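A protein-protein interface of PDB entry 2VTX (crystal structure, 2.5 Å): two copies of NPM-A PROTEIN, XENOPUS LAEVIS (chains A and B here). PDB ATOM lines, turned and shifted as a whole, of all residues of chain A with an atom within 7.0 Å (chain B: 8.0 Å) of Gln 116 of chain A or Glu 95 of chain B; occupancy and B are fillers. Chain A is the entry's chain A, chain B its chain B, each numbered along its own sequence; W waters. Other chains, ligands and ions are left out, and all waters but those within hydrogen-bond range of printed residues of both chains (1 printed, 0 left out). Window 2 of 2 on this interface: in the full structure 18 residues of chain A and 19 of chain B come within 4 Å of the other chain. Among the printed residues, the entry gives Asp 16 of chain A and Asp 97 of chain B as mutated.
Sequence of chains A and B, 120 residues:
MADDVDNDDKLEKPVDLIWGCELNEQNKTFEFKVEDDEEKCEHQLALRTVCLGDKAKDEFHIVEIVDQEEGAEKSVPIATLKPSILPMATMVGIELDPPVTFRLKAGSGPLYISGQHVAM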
ATOM      1  N   ASP A  16     -13.774   9.016  23.331  1.00  0.00           N
ATOM      2  CA  ASP A  16     -14.446   8.318  22.160  1.00  0.00           C
ATOM      3  C   ASP A  16     -13.501   8.086  20.906  1.00  0.00           C
ATOM      4  O   ASP A  16     -12.715   7.072  20.863  1.00  0.00           O
ATOM      5  CB  ASP A  16     -15.843   9.044  21.760  1.00  0.00           C
ATOM      6  N   LEU A  17     -13.562   8.971  19.885  1.00  0.00           N
ATOM      7  CA  LEU A  17     -12.918   8.620  18.555  1.00  0.00           C
ATOM      8  C   LEU A  17     -11.395   8.314  18.816  1.00  0.00           C
ATOM      9  O   LEU A  17     -10.728   9.013  19.697  1.00  0.00           O
ATOM     10  CB  LEU A  17     -13.169   9.713  17.465  1.00  0.00           C
ATOM     11  CG  LEU A  17     -13.300   9.557  15.888  1.00  0.00           C
ATOM     12  CD1 LEU A  17     -14.336  10.607  15.313  1.00  0.00           C
ATOM     13  CD2 LEU A  17     -11.970   9.682  15.021  1.00  0.00           C
ATOM     14  N   ILE A  18     -10.900   7.235  18.159  1.00  0.00           N
ATOM     15  CA  ILE A  18      -9.453   6.914  18.177  1.00  0.00           C
ATOM     16  C   ILE A  18      -8.598   7.940  17.420  1.00  0.00           C
ATOM     17  O   ILE A  18      -8.942   8.388  16.348  1.00  0.00           O
ATOM     18  CB  ILE A  18      -9.174   5.576  17.623  1.00  0.00           C
ATOM     19  CG1 ILE A  18      -7.787   5.089  18.049  1.00  0.00           C
ATOM     20  CG2 ILE A  18      -9.258   5.629  16.194  1.00  0.00           C
ATOM     21  CD1 ILE A  18      -7.789   4.290  19.290  1.00  0.00           C
ATOM     22  N   TRP A  19      -7.461   8.315  17.995  1.00  0.00           N
ATOM     23  CA  TRP A  19      -6.544   9.228  17.377  1.00  0.00           C
ATOM     24  C   TRP A  19      -5.186   8.554  17.115  1.00  0.00           C
ATOM     25  O   TRP A  19      -4.758   7.728  17.819  1.00  0.00           O
ATOM     26  CB  TRP A  19      -6.419  10.436  18.291  1.00  0.00           C
ATOM     27  CG  TRP A  19      -5.300  11.291  17.936  1.00  0.00           C
ATOM     28  CD1 TRP A  19      -5.326  12.334  17.108  1.00  0.00           C
ATOM     29  CD2 TRP A  19      -3.924  11.161  18.344  1.00  0.00           C
ATOM     30  NE1 TRP A  19      -4.098  12.941  17.040  1.00  0.00           N
ATOM     31  CE2 TRP A  19      -3.217  12.223  17.780  1.00  0.00           C
ATOM     32  CE3 TRP A  19      -3.253  10.320  19.194  1.00  0.00           C
ATOM     33  CZ2 TRP A  19      -1.865  12.422  18.000  1.00  0.00           C
ATOM     34  CZ3 TRP A  19      -1.903  10.543  19.401  1.00  0.00           C
ATOM     35  CH2 TRP A  19      -1.230  11.562  18.785  1.00  0.00           C
ATOM     36  N   GLY A  20      -4.469   8.973  16.101  1.00  0.00           N
ATOM     37  CA  GLY A  20      -3.103   8.486  15.906  1.00  0.00           C
ATOM     38  C   GLY A  20      -2.237   9.445  15.109  1.00  0.00           C
ATOM     39  O   GLY A  20      -2.812  10.329  14.482  1.00  0.00           O
ATOM     40  N   GLN A  44      -8.441  15.875  27.617  1.00  0.00           N
ATOM     41  CA  GLN A  44      -7.101  15.318  27.582  1.00  0.00           C
ATOM     42  C   GLN A  44      -6.915  14.384  26.309  1.00  0.00           C
ATOM     43  O   GLN A  44      -7.874  13.970  25.682  1.00  0.00           O
ATOM     44  CB  GLN A  44      -6.777  14.559  28.940  1.00  0.00           C
ATOM     45  CG  GLN A  44      -6.863  15.295  30.403  1.00  0.00           C
ATOM     46  CD  GLN A  44      -5.429  15.657  31.110  1.00  0.00           C
ATOM     47  OE1 GLN A  44      -5.023  15.116  32.211  1.00  0.00           O
ATOM     48  NE2 GLN A  44      -4.695  16.619  30.467  1.00  0.00           N
ATOM     49  N   LEU A  45      -5.669  14.135  25.904  1.00  0.00           N
ATOM     50  CA  LEU A  45      -5.307  13.028  25.065  1.00  0.00           C
ATOM     51  C   LEU A  45      -4.761  11.886  25.938  1.00  0.00           C
ATOM     52  O   LEU A  45      -3.798  12.081  26.667  1.00  0.00           O
ATOM     53  CB  LEU A  45      -4.207  13.441  24.156  1.00  0.00           C
ATOM     54  CG  LEU A  45      -3.773  12.457  23.068  1.00  0.00           C
ATOM     55  CD1 LEU A  45      -5.003  11.915  22.197  1.00  0.00           C
ATOM     56  CD2 LEU A  45      -2.646  13.144  22.255  1.00  0.00           C
ATOM     57  N   ALA A  46      -5.354  10.700  25.866  1.00  0.00           N
ATOM     58  CA  ALA A  46      -4.854   9.534  26.611  1.00  0.00           C
ATOM     59  C   ALA A  46      -4.056   8.628  25.610  1.00  0.00           C
ATOM     60  O   ALA A  46      -4.551   8.233  24.613  1.00  0.00           O
ATOM     61  CB  ALA A  46      -6.054   8.791  27.222  1.00  0.00           C
ATOM     62  N   LEU A  47      -2.819   8.337  25.823  1.00  0.00           N
ATOM     63  CA  LEU A  47      -2.065   7.609  24.832  1.00  0.00           C
ATOM     64  C   LEU A  47      -2.366   6.174  25.028  1.00  0.00           C
ATOM     65  O   LEU A  47      -2.559   5.794  26.135  1.00  0.00           O
ATOM     66  CB  LEU A  47      -0.606   7.880  24.992  1.00  0.00           C
ATOM     67  CG  LEU A  47      -0.207   9.365  24.841  1.00  0.00           C
ATOM     68  CD1 LEU A  47       1.366   9.421  24.912  1.00  0.00           C
ATOM     69  CD2 LEU A  47      -0.798   9.882  23.508  1.00  0.00           C
ATOM     70  N   ARG A  48      -2.491   5.359  24.004  1.00  0.00           N
ATOM     71  CA  ARG A  48      -2.697   3.899  24.272  1.00  0.00           C
ATOM     72  C   ARG A  48      -1.504   2.996  23.914  1.00  0.00           C
ATOM     73  O   ARG A  48      -1.118   2.083  24.665  1.00  0.00           O
ATOM     74  CB  ARG A  48      -3.918   3.391  23.480  1.00  0.00           C
ATOM     75  CG  ARG A  48      -5.251   4.150  23.769  1.00  0.00           C
ATOM     76  CD  ARG A  48      -5.618   4.017  25.176  1.00  0.00           C
ATOM     77  NE  ARG A  48      -6.903   4.617  25.566  1.00  0.00           N
ATOM     78  CZ  ARG A  48      -7.109   5.094  26.800  1.00  0.00           C
ATOM     79  NH1 ARG A  48      -6.147   5.136  27.721  1.00  0.00           N
ATOM     80  NH2 ARG A  48      -8.259   5.611  27.108  1.00  0.00           N
ATOM     81  N   SER A 114      -0.883   5.917  19.213  1.00  0.00           N
ATOM     82  CA  SER A 114      -2.313   5.936  19.113  1.00  0.00           C
ATOM     83  C   SER A 114      -2.752   6.533  20.412  1.00  0.00           C
ATOM     84  O   SER A 114      -2.026   6.418  21.406  1.00  0.00           O
ATOM     85  CB  SER A 114      -2.873   4.532  18.899  1.00  0.00           C
ATOM     86  OG  SER A 114      -2.535   3.701  20.055  1.00  0.00           O
ATOM     87  N   GLY A 115      -3.957   7.152  20.414  1.00  0.00           N
ATOM     88  CA  GLY A 115      -4.544   7.657  21.648  1.00  0.00           C
ATOM     89  C   GLY A 115      -6.048   7.918  21.538  1.00  0.00           C
ATOM     90  O   GLY A 115      -6.674   7.704  20.477  1.00  0.00           O
ATOM     91  N   GLN A 116      -6.639   8.336  22.645  1.00  0.00           N
ATOM     92  CA  GLN A 116      -8.069   8.599  22.718  1.00  0.00           C
ATOM     93  C   GLN A 116      -8.347   9.911  23.427  1.00  0.00           C
ATOM     94  O   GLN A 116      -7.622  10.282  24.330  1.00  0.00           O
ATOM     95  CB  GLN A 116      -8.799   7.428  23.429  1.00  0.00           C
ATOM     96  CG  GLN A 116      -8.928   6.238  22.513  1.00  0.00           C
ATOM     97  CD  GLN A 116      -9.811   5.195  23.040  1.00  0.00           C
ATOM     98  OE1 GLN A 116      -9.494   4.531  24.054  1.00  0.00           O
ATOM     99  NE2 GLN A 116     -10.949   5.036  22.415  1.00  0.00           N
ATOM    100  N   HIS A 117      -9.371  10.636  22.980  1.00  0.00           N
ATOM    101  CA  HIS A 117      -9.841  11.905  23.674  1.00  0.00           C
ATOM    102  C   HIS A 117     -10.543  11.576  25.021  1.00  0.00           C
ATOM    103  O   HIS A 117     -11.458  10.801  25.063  1.00  0.00           O
ATOM    104  CB  HIS A 117     -10.712  12.774  22.748  1.00  0.00           C
ATOM    105  CG  HIS A 117     -10.113  12.982  21.381  1.00  0.00           C
ATOM    106  ND1 HIS A 117      -8.989  13.742  21.165  1.00  0.00           N
ATOM    107  CD2 HIS A 117     -10.450  12.466  20.165  1.00  0.00           C
ATOM    108  CE1 HIS A 117      -8.674  13.712  19.874  1.00  0.00           C
ATOM    109  NE2 HIS A 117      -9.536  12.932  19.245  1.00  0.00           N
ATOM    110  N   VAL A 118     -10.057  12.072  26.138  1.00  0.00           N
ATOM    111  CA  VAL A 118     -10.742  11.735  27.365  1.00  0.00           C
ATOM    112  C   VAL A 118     -10.783  12.877  28.314  1.00  0.00           C
ATOM    113  O   VAL A 118     -11.445  13.837  27.973  1.00  0.00           O
ATOM    114  CB  VAL A 118     -10.127  10.534  28.032  1.00  0.00           C
ATOM    115  CG1 VAL A 118      -9.837   9.477  26.909  1.00  0.00           C
ATOM    116  CG2 VAL A 118      -8.924  10.950  29.027  1.00  0.00           C
ATOM    117  N   GLN B  44     -19.714  -0.277  24.711  1.00  0.00           N
ATOM    118  CA  GLN B  44     -18.414  -0.157  24.080  1.00  0.00           C
ATOM    119  C   GLN B  44     -17.699  -1.479  23.949  1.00  0.00           C
ATOM    120  O   GLN B  44     -18.071  -2.395  24.588  1.00  0.00           O
ATOM    121  CB  GLN B  44     -17.547   0.848  24.834  1.00  0.00           C
ATOM    122  CG  GLN B  44     -18.155   2.259  25.077  1.00  0.00           C
ATOM    123  CD  GLN B  44     -17.047   3.233  25.497  1.00  0.00           C
ATOM    124  OE1 GLN B  44     -16.599   4.078  24.675  1.00  0.00           O
ATOM    125  NE2 GLN B  44     -16.533   3.074  26.744  1.00  0.00           N
ATOM    126  N   LEU B  45     -16.691  -1.607  23.056  1.00  0.00           N
ATOM    127  CA  LEU B  45     -15.871  -2.832  22.984  1.00  0.00           C
ATOM    128  C   LEU B  45     -14.579  -2.436  23.596  1.00  0.00           C
ATOM    129  O   LEU B  45     -13.997  -1.457  23.204  1.00  0.00           O
ATOM    130  CB  LEU B  45     -15.630  -3.175  21.559  1.00  0.00           C
ATOM    131  CG  LEU B  45     -14.756  -4.400  21.313  1.00  0.00           C
ATOM    132  CD1 LEU B  45     -15.278  -5.732  21.957  1.00  0.00           C
ATOM    133  CD2 LEU B  45     -14.596  -4.558  19.830  1.00  0.00           C
ATOM    134  N   ALA B  46     -14.181  -3.090  24.663  1.00  0.00           N
ATOM    135  CA  ALA B  46     -12.909  -2.813  25.344  1.00  0.00           C
ATOM    136  C   ALA B  46     -11.907  -3.871  24.949  1.00  0.00           C
ATOM    137  O   ALA B  46     -12.144  -5.041  25.213  1.00  0.00           O
ATOM    138  CB  ALA B  46     -13.068  -2.831  26.915  1.00  0.00           C
ATOM    139  N   LEU B  47     -10.786  -3.474  24.341  1.00  0.00           N
ATOM    140  CA  LEU B  47      -9.798  -4.439  23.833  1.00  0.00           C
ATOM    141  C   LEU B  47      -9.065  -5.011  24.984  1.00  0.00           C
ATOM    142  O   LEU B  47      -8.936  -4.387  25.976  1.00  0.00           O
ATOM    143  CB  LEU B  47      -8.818  -3.824  22.902  1.00  0.00           C
ATOM    144  CG  LEU B  47      -9.394  -3.297  21.578  1.00  0.00           C
ATOM    145  CD1 LEU B  47      -8.279  -3.005  20.547  1.00  0.00           C
ATOM    146  CD2 LEU B  47     -10.465  -4.292  21.003  1.00  0.00           C
ATOM    147  N   ARG B  48      -8.687  -6.271  24.904  1.00  0.00           N
ATOM    148  CA  ARG B  48      -7.901  -6.814  25.984  1.00  0.00           C
ATOM    149  C   ARG B  48      -6.504  -7.309  25.565  1.00  0.00           C
ATOM    150  O   ARG B  48      -5.560  -7.043  26.245  1.00  0.00           O
ATOM    151  CB  ARG B  48      -8.674  -7.964  26.659  1.00  0.00           C
ATOM    152  CG  ARG B  48      -9.896  -7.605  27.316  1.00  0.00           C
ATOM    153  CD  ARG B  48      -9.742  -6.843  28.582  1.00  0.00           C
ATOM    154  NE  ARG B  48     -11.093  -6.484  29.108  1.00  0.00           N
ATOM    155  CZ  ARG B  48     -11.462  -5.231  29.446  1.00  0.00           C
ATOM    156  NH1 ARG B  48     -10.645  -4.156  29.343  1.00  0.00           N
ATOM    157  NH2 ARG B  48     -12.706  -5.049  29.857  1.00  0.00           N
ATOM    158  N   ILE B  65      -6.882   0.330  13.490  1.00  0.00           N
ATOM    159  CA  ILE B  65      -8.267   0.709  13.499  1.00  0.00           C
ATOM    160  C   ILE B  65      -8.587   1.627  12.304  1.00  0.00           C
ATOM    161  O   ILE B  65      -7.926   2.614  12.025  1.00  0.00           O
ATOM    162  CB  ILE B  65      -8.654   1.317  14.826  1.00  0.00           C
ATOM    163  CG1 ILE B  65      -8.640   0.295  15.908  1.00  0.00           C
ATOM    164  CG2 ILE B  65     -10.133   1.839  14.812  1.00  0.00           C
ATOM    165  CD1 ILE B  65      -8.468   0.859  17.297  1.00  0.00           C
ATOM    166  N   VAL B  92      -4.603  -1.875  26.975  1.00  0.00           N
ATOM    167  CA  VAL B  92      -5.119  -1.253  28.178  1.00  0.00           C
ATOM    168  C   VAL B  92      -5.789   0.078  27.810  1.00  0.00           C
ATOM    169  O   VAL B  92      -5.180   0.927  27.149  1.00  0.00           O
ATOM    170  CB  VAL B  92      -3.973  -1.029  29.186  1.00  0.00           C
ATOM    171  CG1 VAL B  92      -4.507  -0.294  30.477  1.00  0.00           C
ATOM    172  CG2 VAL B  92      -3.243  -2.391  29.524  1.00  0.00           C
ATOM    173  N   GLY B  93      -7.026   0.253  28.260  1.00  0.00           N
ATOM    174  CA  GLY B  93      -7.719   1.500  28.199  1.00  0.00           C
ATOM    175  C   GLY B  93      -8.343   1.691  26.844  1.00  0.00           C
ATOM    176  O   GLY B  93      -9.050   2.659  26.632  1.00  0.00           O
ATOM    177  N   ILE B  94      -8.129   0.818  25.871  1.00  0.00           N
ATOM    178  CA  ILE B  94      -8.799   1.113  24.568  1.00  0.00           C
ATOM    179  C   ILE B  94     -10.265   0.723  24.659  1.00  0.00           C
ATOM    180  O   ILE B  94     -10.570  -0.448  24.712  1.00  0.00           O
ATOM    181  CB  ILE B  94      -8.121   0.466  23.359  1.00  0.00           C
ATOM    182  CG1 ILE B  94      -6.653   0.900  23.311  1.00  0.00           C
ATOM    183  CG2 ILE B  94      -8.709   0.996  22.181  1.00  0.00           C
ATOM    184  CD1 ILE B  94      -5.750   0.183  22.379  1.00  0.00           C
ATOM    185  N   GLU B  95     -11.166   1.698  24.651  1.00  0.00           N
ATOM    186  CA  GLU B  95     -12.621   1.407  24.625  1.00  0.00           C
ATOM    187  C   GLU B  95     -13.171   2.058  23.447  1.00  0.00           C
ATOM    188  O   GLU B  95     -12.961   3.213  23.268  1.00  0.00           O
ATOM    189  CB  GLU B  95     -13.367   1.872  25.845  1.00  0.00           C
ATOM    190  CG  GLU B  95     -12.477   1.841  27.010  1.00  0.00           C
ATOM    191  CD  GLU B  95     -13.156   1.497  28.292  1.00  0.00           C
ATOM    192  OE1 GLU B  95     -13.890   2.408  28.814  1.00  0.00           O
ATOM    193  OE2 GLU B  95     -12.876   0.348  28.779  1.00  0.00           O
ATOM    194  N   LEU B  96     -13.882   1.304  22.627  1.00  0.00           N
ATOM    195  CA  LEU B  96     -14.333   1.827  21.379  1.00  0.00           C
ATOM    196  C   LEU B  96     -15.803   1.816  21.276  1.00  0.00           C
ATOM    197  O   LEU B  96     -16.494   0.927  21.790  1.00  0.00           O
ATOM    198  CB  LEU B  96     -13.767   0.999  20.241  1.00  0.00           C
ATOM    199  CG  LEU B  96     -12.237   1.064  20.103  1.00  0.00           C
ATOM    200  CD1 LEU B  96     -11.718  -0.198  19.356  1.00  0.00           C
ATOM    201  CD2 LEU B  96     -11.841   2.387  19.484  1.00  0.00           C
ATOM    202  N   ASP B  97     -16.259   2.770  20.487  1.00  0.00           N
ATOM    203  CA  ASP B  97     -17.634   2.874  20.030  1.00  0.00           C
ATOM    204  C   ASP B  97     -17.924   2.131  18.786  1.00  0.00           C
ATOM    205  O   ASP B  97     -17.501   2.537  17.763  1.00  0.00           O
ATOM    206  CB  ASP B  97     -17.946   4.330  19.725  1.00  0.00           C
ATOM    207  CG  ASP B  97     -19.013   4.877  20.616  1.00  0.00           C
ATOM    208  OD1 ASP B  97     -20.211   4.388  20.481  1.00  0.00           O
ATOM    209  OD2 ASP B  97     -18.608   5.770  21.426  1.00  0.00           O
ATOM    210  N   PRO B  98     -18.760   1.103  18.850  1.00  0.00           N
ATOM    211  CA  PRO B  98     -19.161   0.433  17.661  1.00  0.00           C
ATOM    212  C   PRO B  98     -19.840   1.416  16.705  1.00  0.00           C
ATOM    213  O   PRO B  98     -20.530   2.338  17.137  1.00  0.00           O
ATOM    214  CB  PRO B  98     -20.235  -0.514  18.172  1.00  0.00           C
ATOM    215  CG  PRO B  98     -20.010  -0.682  19.630  1.00  0.00           C
ATOM    216  CD  PRO B  98     -19.512   0.629  20.024  1.00  0.00           C
ATOM    217  N   VAL B 100     -16.730  -0.595  14.682  1.00  0.00           N
ATOM    218  CA  VAL B 100     -15.322  -0.459  14.624  1.00  0.00           C
ATOM    219  C   VAL B 100     -14.794  -1.378  13.604  1.00  0.00           C
ATOM    220  O   VAL B 100     -15.168  -2.518  13.630  1.00  0.00           O
ATOM    221  CB  VAL B 100     -14.683  -0.946  15.920  1.00  0.00           C
ATOM    222  CG1 VAL B 100     -13.346  -0.417  15.952  1.00  0.00           C
ATOM    223  CG2 VAL B 100     -15.455  -0.520  17.188  1.00  0.00           C
ATOM    224  N   GLN B 116     -13.972  -7.252  25.430  1.00  0.00           N
ATOM    225  CA  GLN B 116     -15.114  -7.441  26.216  1.00  0.00           C
ATOM    226  C   GLN B 116     -16.100  -6.352  26.016  1.00  0.00           C
ATOM    227  O   GLN B 116     -15.754  -5.243  25.808  1.00  0.00           O
ATOM    228  CB  GLN B 116     -14.733  -7.493  27.696  1.00  0.00           C
ATOM    229  CG  GLN B 116     -14.055  -8.737  28.032  1.00  0.00           C
ATOM    230  CD  GLN B 116     -13.769  -8.910  29.483  1.00  0.00           C
ATOM    231  OE1 GLN B 116     -12.866  -8.238  30.031  1.00  0.00           O
ATOM    232  NE2 GLN B 116     -14.475  -9.882  30.120  1.00  0.00           N
ATOM    233  N   HIS B 117     -17.370  -6.689  26.227  1.00  0.00           N
ATOM    234  CA  HIS B 117     -18.446  -5.674  26.328  1.00  0.00           C
ATOM    235  C   HIS B 117     -18.400  -4.845  27.601  1.00  0.00           C
ATOM    236  O   HIS B 117     -18.081  -5.321  28.657  1.00  0.00           O
ATOM    237  CB  HIS B 117     -19.753  -6.354  26.006  1.00  0.00           C
ATOM    238  CG  HIS B 117     -19.709  -6.991  24.640  1.00  0.00           C
ATOM    239  ND1 HIS B 117     -19.541  -6.242  23.495  1.00  0.00           N
ATOM    240  CD2 HIS B 117     -19.671  -8.289  24.248  1.00  0.00           C
ATOM    241  CE1 HIS B 117     -19.477  -7.058  22.444  1.00  0.00           C
ATOM    242  NE2 HIS B 117     -19.572  -8.306  22.868  1.00  0.00           N
ATOM    243  N   VAL B 118     -18.606  -3.550  27.456  1.00  0.00           N
ATOM    244  CA  VAL B 118     -18.446  -2.665  28.566  1.00  0.00           C
ATOM    245  C   VAL B 118     -19.616  -1.640  28.596  1.00  0.00           C
ATOM    246  O   VAL B 118     -20.090  -1.181  27.549  1.00  0.00           O
ATOM    247  CB  VAL B 118     -16.962  -2.168  28.536  1.00  0.00           C
ATOM    248  CG1 VAL B 118     -16.797  -0.671  28.538  1.00  0.00           C
ATOM    249  CG2 VAL B 118     -16.137  -2.906  29.623  1.00  0.00           C
ATOM    250  N   ALA B 119     -20.137  -1.329  29.785  1.00  0.00           N
ATOM    251  CA  ALA B 119     -21.298  -0.343  29.894  1.00  0.00           C
ATOM    252  C   ALA B 119     -20.857   0.963  30.557  1.00  0.00           C
ATOM    253  O   ALA B 119     -20.110   1.736  29.928  1.00  0.00           O
ATOM    254  CB  ALA B 119     -22.535  -0.960  30.633  1.00  0.00           C
HETATM  255  O   HOH W   1      -3.682   3.188  28.050  1.00  0.00           O
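The guanidinium group (NH2) of Arg 48 of chain A is in hydrogen-bond range of the backbone carbonyl oxygen (O) of Gly 93 of chain B (3.1 Å). The side-chain amide oxygen of Gln 116 of chain A lies close to the backbone carbonyl oxygen of Gly 93 of chain B, at 3.2 Å. The backbone carbonyl oxygen (O) of Glu 95 of chain B lies within hydrogen-bond range of the side-chain amide nitrogen (NE2) of Gln 116 of chain A, 2.8 Å away.
The backbone carbonyl oxygen (O) of Asp 16 of chain A lies within hydrogen-bond range of the side-chain amide nitrogen (NE2) of Gln 116 of chain A (3.1 Å). N of Ala 46 of chain A sits at hydrogen-bond distance from O of Gln 116 of chain A, 2.8 Å away. The backbone NH (N) of Arg 48 of chain A is in hydrogen-bond range of the backbone carbonyl oxygen (O) of Ser 114 of chain A, at 2.8 Å. The side-chain amide oxygen (OE1) of Gln 116 of chain A lies within hydrogen-bond range of the guanidinium group (NE) of Arg 48 of chain A. The side-chain amide nitrogen (NE2) of Gln 44 of chain B is in hydrogen-bond range of the side-chain carboxylate (OE1) of Glu 95 of chain B (3.4 Å). N of Leu 47 of chain B is in hydrogen-bond range of O of Ile 94 of chain B (3.1 Å).
Val 92 of chain B touches Arg 48 of chain A (O to CD, 3.7 Å). Arg 48 of chain A touches Ile 94 of chain B. Ile 94 of chain B touches Gln 116 of chain A.
Of chain B, only Gly 93, Ile 94 and Glu 95 come within 4 Å of Gln 116 of chain A. Glu 95 of chain B touches one residue of chain A. No residue of chain B comes within 4 Å of Ala 46 of chain A. No residue of chain B comes within 4 Å of Gly 115 of chain A. Of the printed residues of chain A, Ile 94 of chain B touches Arg 48 (3.6 Å) and Gln 116 (3.5 Å). Printed residues of chain A within 4 Å of Val 92 of chain B: Arg 48 (3.7 Å). Of the printed residues of chain A, Gly 93 of chain B touches Arg 48 and Gln 116. Of the printed residues of chain B, Arg 48 of chain A touches Val 92, Gly 93 and Ile 94. Leu 47 of chain A touches none of the printed residues of chain B. Trp 19 of chain A touches none of the printed residues of chain B. The nearest printed residue of chain A that does not touch Gly 93 of chain B is Ala 46 of chain A (6.9 Å).
Of the 18 printed residues of chain B, 4 touch a printed residue of chain A. Printed residues of chain B that touch a printed residue of chain A: Val 92, Gly 93, Ile 94 and Glu 95. Among the printed residues, no Asp or Glu carboxylate lies within 4 Å of a Lys or Arg side-chain nitrogen of the other chain.
Positions printed for both chains: 44, 45, 46, 47, 48, 116, 117 and 118. Of the 6 pairs that touch across the chains among the printed residues, none has its exchanged pair printed and touching as well.
Water W1 lies within hydrogen-bond range of the backbone carbonyl oxygen of Val 92 of chain B, the guanidinium group of Arg 48 of chain A and the backbone carbonyl oxygen of Leu 47 of chain A.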
